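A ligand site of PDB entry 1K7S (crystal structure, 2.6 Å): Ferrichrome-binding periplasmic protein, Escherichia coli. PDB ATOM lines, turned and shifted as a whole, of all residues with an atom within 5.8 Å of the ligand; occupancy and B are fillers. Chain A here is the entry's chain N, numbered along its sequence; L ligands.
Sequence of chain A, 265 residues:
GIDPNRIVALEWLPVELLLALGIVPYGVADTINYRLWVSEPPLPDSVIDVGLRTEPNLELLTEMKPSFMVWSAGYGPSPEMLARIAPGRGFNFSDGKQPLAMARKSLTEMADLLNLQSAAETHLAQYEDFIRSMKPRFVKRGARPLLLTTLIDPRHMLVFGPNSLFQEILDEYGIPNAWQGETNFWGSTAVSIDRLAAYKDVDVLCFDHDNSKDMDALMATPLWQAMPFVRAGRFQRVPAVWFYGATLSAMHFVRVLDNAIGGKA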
ATOM      1  N   GLU A  11      30.066 -28.859  25.586  1.00  0.00           N
ATOM      2  CA  GLU A  11      29.283 -29.089  24.387  1.00  0.00           C
ATOM      3  C   GLU A  11      28.989 -30.586  24.360  1.00  0.00           C
ATOM      4  O   GLU A  11      29.761 -31.366  24.913  1.00  0.00           O
ATOM      5  CB  GLU A  11      30.079 -28.685  23.152  1.00  0.00           C
ATOM      6  CG  GLU A  11      29.238 -28.059  22.047  1.00  0.00           C
ATOM      7  CD  GLU A  11      28.294 -29.044  21.375  1.00  0.00           C
ATOM      8  OE1 GLU A  11      28.779 -30.010  20.746  1.00  0.00           O
ATOM      9  OE2 GLU A  11      27.076 -28.838  21.479  1.00  0.00           O
ATOM     10  N   TRP A  12      27.896 -30.976  23.707  1.00  0.00           N
ATOM     11  CA  TRP A  12      27.494 -32.374  23.656  1.00  0.00           C
ATOM     12  C   TRP A  12      28.297 -33.286  22.740  1.00  0.00           C
ATOM     13  O   TRP A  12      28.114 -34.496  22.757  1.00  0.00           O
ATOM     14  CB  TRP A  12      25.997 -32.474  23.323  1.00  0.00           C
ATOM     15  CG  TRP A  12      25.135 -31.629  24.229  1.00  0.00           C
ATOM     16  CD1 TRP A  12      25.413 -31.283  25.526  1.00  0.00           C
ATOM     17  CD2 TRP A  12      23.901 -30.990  23.903  1.00  0.00           C
ATOM     18  NE1 TRP A  12      24.436 -30.455  26.024  1.00  0.00           N
ATOM     19  CE2 TRP A  12      23.496 -30.266  25.045  1.00  0.00           C
ATOM     20  CE3 TRP A  12      23.094 -30.953  22.764  1.00  0.00           C
ATOM     21  CZ2 TRP A  12      22.313 -29.505  25.081  1.00  0.00           C
ATOM     22  CZ3 TRP A  12      21.918 -30.202  22.788  1.00  0.00           C
ATOM     23  CH2 TRP A  12      21.544 -29.493  23.944  1.00  0.00           C
ATOM     24  N   TRP A  37      17.441 -33.486  23.192  1.00  0.00           N
ATOM     25  CA  TRP A  37      18.085 -33.652  21.884  1.00  0.00           C
ATOM     26  C   TRP A  37      19.033 -34.840  21.733  1.00  0.00           C
ATOM     27  O   TRP A  37      19.038 -35.495  20.696  1.00  0.00           O
ATOM     28  CB  TRP A  37      18.812 -32.372  21.495  1.00  0.00           C
ATOM     29  CG  TRP A  37      17.943 -31.180  21.388  1.00  0.00           C
ATOM     30  CD1 TRP A  37      17.615 -30.323  22.387  1.00  0.00           C
ATOM     31  CD2 TRP A  37      17.348 -30.665  20.194  1.00  0.00           C
ATOM     32  NE1 TRP A  37      16.867 -29.275  21.886  1.00  0.00           N
ATOM     33  CE2 TRP A  37      16.684 -29.466  20.544  1.00  0.00           C
ATOM     34  CE3 TRP A  37      17.307 -31.093  18.853  1.00  0.00           C
ATOM     35  CZ2 TRP A  37      16.002 -28.694  19.607  1.00  0.00           C
ATOM     36  CZ3 TRP A  37      16.623 -30.319  17.929  1.00  0.00           C
ATOM     37  CH2 TRP A  37      15.984 -29.124  18.305  1.00  0.00           C
ATOM     38  N   ARG A  53      25.639 -23.982  26.719  1.00  0.00           N
ATOM     39  CA  ARG A  53      26.904 -24.178  26.012  1.00  0.00           C
ATOM     40  C   ARG A  53      27.398 -22.855  25.437  1.00  0.00           C
ATOM     41  O   ARG A  53      28.602 -22.641  25.289  1.00  0.00           O
ATOM     42  CB  ARG A  53      26.737 -25.214  24.911  1.00  0.00           C
ATOM     43  CG  ARG A  53      26.183 -26.540  25.408  1.00  0.00           C
ATOM     44  CD  ARG A  53      24.842 -26.840  24.759  1.00  0.00           C
ATOM     45  NE  ARG A  53      25.017 -27.311  23.394  1.00  0.00           N
ATOM     46  CZ  ARG A  53      24.131 -27.150  22.419  1.00  0.00           C
ATOM     47  NH1 ARG A  53      22.990 -26.525  22.664  1.00  0.00           N
ATOM     48  NH2 ARG A  53      24.387 -27.633  21.211  1.00  0.00           N
ATOM     49  N   THR A  54      26.462 -21.977  25.129  1.00  0.00           N
ATOM     50  CA  THR A  54      26.770 -20.681  24.556  1.00  0.00           C
ATOM     51  C   THR A  54      27.224 -19.653  25.572  1.00  0.00           C
ATOM     52  O   THR A  54      28.103 -18.846  25.283  1.00  0.00           O
ATOM     53  CB  THR A  54      25.564 -20.096  23.795  1.00  0.00           C
ATOM     54  OG1 THR A  54      24.386 -20.250  24.587  1.00  0.00           O
ATOM     55  CG2 THR A  54      25.393 -20.808  22.465  1.00  0.00           C
ATOM     56  N   TYR A  75      32.347 -23.408  18.084  1.00  0.00           N
ATOM     57  CA  TYR A  75      31.063 -23.250  18.773  1.00  0.00           C
ATOM     58  C   TYR A  75      31.277 -22.809  20.228  1.00  0.00           C
ATOM     59  O   TYR A  75      32.288 -23.137  20.849  1.00  0.00           O
ATOM     60  CB  TYR A  75      30.289 -24.568  18.758  1.00  0.00           C
ATOM     61  CG  TYR A  75      28.916 -24.466  19.409  1.00  0.00           C
ATOM     62  CD1 TYR A  75      27.789 -24.076  18.669  1.00  0.00           C
ATOM     63  CD2 TYR A  75      28.754 -24.728  20.763  1.00  0.00           C
ATOM     64  CE1 TYR A  75      26.541 -23.951  19.282  1.00  0.00           C
ATOM     65  CE2 TYR A  75      27.517 -24.607  21.385  1.00  0.00           C
ATOM     66  CZ  TYR A  75      26.413 -24.218  20.641  1.00  0.00           C
ATOM     67  OH  TYR A  75      25.187 -24.103  21.258  1.00  0.00           O
ATOM     68  N   THR A 150      14.091 -32.753  10.979  1.00  0.00           N
ATOM     69  CA  THR A 150      13.678 -32.451  12.351  1.00  0.00           C
ATOM     70  C   THR A 150      13.033 -31.066  12.274  1.00  0.00           C
ATOM     71  O   THR A 150      13.509 -30.195  11.535  1.00  0.00           O
ATOM     72  CB  THR A 150      14.845 -32.420  13.371  1.00  0.00           C
ATOM     73  OG1 THR A 150      14.313 -32.330  14.699  1.00  0.00           O
ATOM     74  CG2 THR A 150      15.751 -31.231  13.129  1.00  0.00           C
ATOM     75  N   ILE A 152      12.122 -27.387  13.480  1.00  0.00           N
ATOM     76  CA  ILE A 152      12.665 -26.302  14.295  1.00  0.00           C
ATOM     77  C   ILE A 152      11.521 -25.397  14.759  1.00  0.00           C
ATOM     78  O   ILE A 152      11.548 -24.837  15.859  1.00  0.00           O
ATOM     79  CB  ILE A 152      13.685 -25.472  13.492  1.00  0.00           C
ATOM     80  CG1 ILE A 152      14.806 -26.393  13.013  1.00  0.00           C
ATOM     81  CG2 ILE A 152      14.245 -24.347  14.338  1.00  0.00           C
ATOM     82  CD1 ILE A 152      15.483 -27.195  14.129  1.00  0.00           C
ATOM     83  N   LEU A 158      14.660 -28.923   9.329  1.00  0.00           N
ATOM     84  CA  LEU A 158      16.084 -29.056   9.079  1.00  0.00           C
ATOM     85  C   LEU A 158      16.221 -30.335   8.280  1.00  0.00           C
ATOM     86  O   LEU A 158      15.601 -31.345   8.599  1.00  0.00           O
ATOM     87  CB  LEU A 158      16.881 -29.189  10.370  1.00  0.00           C
ATOM     88  CG  LEU A 158      17.521 -27.959  10.991  1.00  0.00           C
ATOM     89  CD1 LEU A 158      18.586 -28.427  11.982  1.00  0.00           C
ATOM     90  CD2 LEU A 158      18.169 -27.107   9.937  1.00  0.00           C
ATOM     91  N   ASN A 184      25.235 -26.495   5.833  1.00  0.00           N
ATOM     92  CA  ASN A 184      26.274 -25.733   6.518  1.00  0.00           C
ATOM     93  C   ASN A 184      27.421 -26.694   6.844  1.00  0.00           C
ATOM     94  O   ASN A 184      27.394 -27.871   6.456  1.00  0.00           O
ATOM     95  CB  ASN A 184      25.739 -25.109   7.820  1.00  0.00           C
ATOM     96  CG  ASN A 184      25.019 -26.116   8.719  1.00  0.00           C
ATOM     97  OD1 ASN A 184      25.344 -27.303   8.729  1.00  0.00           O
ATOM     98  ND2 ASN A 184      24.055 -25.645   9.488  1.00  0.00           N
ATOM     99  N   TRP A 186      28.043 -28.147   9.436  1.00  0.00           N
ATOM    100  CA  TRP A 186      27.547 -29.226  10.267  1.00  0.00           C
ATOM    101  C   TRP A 186      26.706 -30.283   9.548  1.00  0.00           C
ATOM    102  O   TRP A 186      26.232 -31.225  10.177  1.00  0.00           O
ATOM    103  CB  TRP A 186      26.752 -28.630  11.433  1.00  0.00           C
ATOM    104  CG  TRP A 186      27.548 -27.642  12.201  1.00  0.00           C
ATOM    105  CD1 TRP A 186      27.813 -26.340  11.854  1.00  0.00           C
ATOM    106  CD2 TRP A 186      28.268 -27.882  13.407  1.00  0.00           C
ATOM    107  NE1 TRP A 186      28.649 -25.769  12.770  1.00  0.00           N
ATOM    108  CE2 TRP A 186      28.945 -26.689  13.743  1.00  0.00           C
ATOM    109  CE3 TRP A 186      28.406 -28.994  14.256  1.00  0.00           C
ATOM    110  CZ2 TRP A 186      29.759 -26.573  14.879  1.00  0.00           C
ATOM    111  CZ3 TRP A 186      29.207 -28.885  15.392  1.00  0.00           C
ATOM    112  CH2 TRP A 186      29.873 -27.684  15.688  1.00  0.00           C
ATOM    113  N   SER A 188      23.776 -29.704   7.738  1.00  0.00           N
ATOM    114  CA  SER A 188      22.338 -29.492   7.626  1.00  0.00           C
ATOM    115  C   SER A 188      21.941 -28.095   7.144  1.00  0.00           C
ATOM    116  O   SER A 188      22.775 -27.212   6.981  1.00  0.00           O
ATOM    117  CB  SER A 188      21.654 -29.766   8.961  1.00  0.00           C
ATOM    118  OG  SER A 188      22.047 -28.815   9.931  1.00  0.00           O
ATOM    119  N   TRP A 242      21.044 -37.067  18.414  1.00  0.00           N
ATOM    120  CA  TRP A 242      21.867 -35.860  18.238  1.00  0.00           C
ATOM    121  C   TRP A 242      22.557 -35.838  16.889  1.00  0.00           C
ATOM    122  O   TRP A 242      23.341 -36.737  16.567  1.00  0.00           O
ATOM    123  CB  TRP A 242      22.920 -35.754  19.339  1.00  0.00           C
ATOM    124  CG  TRP A 242      23.588 -34.419  19.368  1.00  0.00           C
ATOM    125  CD1 TRP A 242      24.904 -34.150  19.593  1.00  0.00           C
ATOM    126  CD2 TRP A 242      22.950 -33.146  19.189  1.00  0.00           C
ATOM    127  NE1 TRP A 242      25.130 -32.794  19.564  1.00  0.00           N
ATOM    128  CE2 TRP A 242      23.944 -32.158  19.317  1.00  0.00           C
ATOM    129  CE3 TRP A 242      21.626 -32.747  18.929  1.00  0.00           C
ATOM    130  CZ2 TRP A 242      23.663 -30.791  19.187  1.00  0.00           C
ATOM    131  CZ3 TRP A 242      21.347 -31.399  18.810  1.00  0.00           C
ATOM    132  CH2 TRP A 242      22.361 -30.435  18.937  1.00  0.00           C
ATOM    133  N   PHE A 243      22.315 -34.789  16.102  1.00  0.00           N
ATOM    134  CA  PHE A 243      22.907 -34.677  14.769  1.00  0.00           C
ATOM    135  C   PHE A 243      24.359 -34.224  14.690  1.00  0.00           C
ATOM    136  O   PHE A 243      24.992 -34.356  13.649  1.00  0.00           O
ATOM    137  CB  PHE A 243      22.074 -33.732  13.921  1.00  0.00           C
ATOM    138  CG  PHE A 243      20.699 -33.498  14.448  1.00  0.00           C
ATOM    139  CD1 PHE A 243      20.339 -32.249  14.972  1.00  0.00           C
ATOM    140  CD2 PHE A 243      19.752 -34.519  14.419  1.00  0.00           C
ATOM    141  CE1 PHE A 243      19.064 -32.019  15.455  1.00  0.00           C
ATOM    142  CE2 PHE A 243      18.469 -34.304  14.903  1.00  0.00           C
ATOM    143  CZ  PHE A 243      18.122 -33.049  15.427  1.00  0.00           C
ATOM    144  N   TYR A 244      24.879 -33.672  15.788  1.00  0.00           N
ATOM    145  CA  TYR A 244      26.245 -33.184  15.808  1.00  0.00           C
ATOM    146  C   TYR A 244      27.126 -33.911  16.835  1.00  0.00           C
ATOM    147  O   TYR A 244      28.043 -33.320  17.411  1.00  0.00           O
ATOM    148  CB  TYR A 244      26.207 -31.679  16.068  1.00  0.00           C
ATOM    149  CG  TYR A 244      25.154 -30.971  15.240  1.00  0.00           C
ATOM    150  CD1 TYR A 244      24.039 -30.387  15.841  1.00  0.00           C
ATOM    151  CD2 TYR A 244      25.226 -30.974  13.840  1.00  0.00           C
ATOM    152  CE1 TYR A 244      23.022 -29.810  15.069  1.00  0.00           C
ATOM    153  CE2 TYR A 244      24.219 -30.403  13.063  1.00  0.00           C
ATOM    154  CZ  TYR A 244      23.125 -29.827  13.683  1.00  0.00           C
ATOM    155  OH  TYR A 244      22.121 -29.276  12.916  1.00  0.00           O
HETATM  156  C1  LIG L   1      20.541 -27.475  19.207  1.00  0.00           C
HETATM  157  C2  LIG L   1      21.256 -25.478  13.493  1.00  0.00           C
HETATM  158  C3  LIG L   1      25.124 -26.807  17.635  1.00  0.00           C
HETATM  159  C4  LIG L   1      23.029 -22.847  13.778  1.00  0.00           C
HETATM  160  C5  LIG L   1      22.643 -23.157  19.317  1.00  0.00           C
HETATM  161  C6  LIG L   1      19.086 -25.428  14.612  1.00  0.00           C
HETATM  162  C7  LIG L   1      22.778 -25.257  13.549  1.00  0.00           C
HETATM  163  C8  LIG L   1      23.436 -21.677  14.669  1.00  0.00           C
HETATM  164  C9  LIG L   1      18.730 -26.283  15.841  1.00  0.00           C
HETATM  165  C10 LIG L   1      23.483 -26.486  14.156  1.00  0.00           C
HETATM  166  C11 LIG L   1      22.923 -21.840  16.101  1.00  0.00           C
HETATM  167  C12 LIG L   1      19.218 -27.707  15.709  1.00  0.00           C
HETATM  168  C13 LIG L   1      25.024 -26.418  14.154  1.00  0.00           C
HETATM  169  C14 LIG L   1      21.422 -21.680  16.293  1.00  0.00           C
HETATM  170  C15 LIG L   1      19.526 -28.371  17.059  1.00  0.00           C
HETATM  171  C16 LIG L   1      25.623 -25.722  15.395  1.00  0.00           C
HETATM  172  C17 LIG L   1      21.009 -21.958  17.749  1.00  0.00           C
HETATM  173  C18 LIG L   1      26.374 -27.644  17.960  1.00  0.00           C
HETATM  174  C19 LIG L   1      19.596 -28.099  20.273  1.00  0.00           C
HETATM  175  C20 LIG L   1      23.108 -21.877  20.053  1.00  0.00           C
HETATM  176  C21 LIG L   1      18.315 -24.112  14.619  1.00  0.00           C
HETATM  177  C22 LIG L   1      18.236 -21.806  13.914  1.00  0.00           C
HETATM  178  C23 LIG L   1      19.145 -20.766  13.328  1.00  0.00           C
HETATM  179 FE1  LIG L   1      22.618 -25.777  18.278  1.00  0.00          FE
HETATM  180  N1  LIG L   1      20.541 -25.195  14.571  1.00  0.00           N
HETATM  181  N2  LIG L   1      23.117 -24.057  14.319  1.00  0.00           N
HETATM  182  N3  LIG L   1      20.471 -27.593  17.875  1.00  0.00           N
HETATM  183  N4  LIG L   1      24.855 -25.997  16.626  1.00  0.00           N
HETATM  184  N5  LIG L   1      21.741 -23.101  18.322  1.00  0.00           N
HETATM  185  N6  LIG L   1      18.883 -23.089  13.980  1.00  0.00           N
HETATM  186  N7  LIG L   1      22.898 -20.445  14.090  1.00  0.00           N
HETATM  187  O1  LIG L   1      21.456 -26.723  19.683  1.00  0.00           O
HETATM  188  O2  LIG L   1      20.736 -25.898  12.468  1.00  0.00           O
HETATM  189  O3  LIG L   1      24.261 -26.871  18.595  1.00  0.00           O
HETATM  190  O4  LIG L   1      22.661 -22.668  12.611  1.00  0.00           O
HETATM  191  O5  LIG L   1      23.142 -24.310  19.582  1.00  0.00           O
HETATM  192  O6  LIG L   1      21.403 -26.888  17.133  1.00  0.00           O
HETATM  193  O7  LIG L   1      23.684 -25.260  16.725  1.00  0.00           O
HETATM  194  O8  LIG L   1      21.408 -24.278  17.730  1.00  0.00           O
HETATM  195  O9  LIG L   1      17.236 -24.029  15.172  1.00  0.00           O
HETATM  196  O10 LIG L   1      20.342 -20.946  13.181  1.00  0.00           O
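An oxygen (O5) of the ligand lies close to the side-chain hydroxyl of Tyr 75, at 2.7 Å.
An oxygen (O3) of the ligand sits close to the guanidinium group of Arg 53.
The guanidinium group of Arg 53 is in salt-bridge range of the side-chain carboxylate of Glu 11, 3.0 Å away.
The backbone carbonyl oxygen of Trp 37 lies within hydrogen-bond range of the backbone NH of Trp 242, at 3.4 Å.
The side-chain hydroxyl (OH) of Tyr 244 sits at hydrogen-bond distance from the side-chain hydroxyl (OG) of Ser 188 (3.0 Å).
N of Leu 158 lies within hydrogen-bond range of O of Thr 150.
OD1 of Asn 184 is in hydrogen-bond range of N of Trp 186 (2.9 Å).
Residues that only touch the ligand: Ile 152 (3.1 Å), Trp 37 (3.2 Å), Tyr 244 (3.3 Å), Leu 158 (3.4 Å), Trp 186 (3.4 Å), Trp 242 (3.5 Å), Thr 54 (3.5 Å) and Glu 11 (3.8 Å).
Hydrophobic or aromatic side chains within 4 Å of the ligand: Trp 37, Tyr 75, Ile 152, Leu 158, Trp 186, Trp 242 and Tyr 244.
Of the 15 residues printed, 10 come within 4 Å of the ligand.
The nearest printed residue that does not touch the ligand is Phe 243 (4.01 Å).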
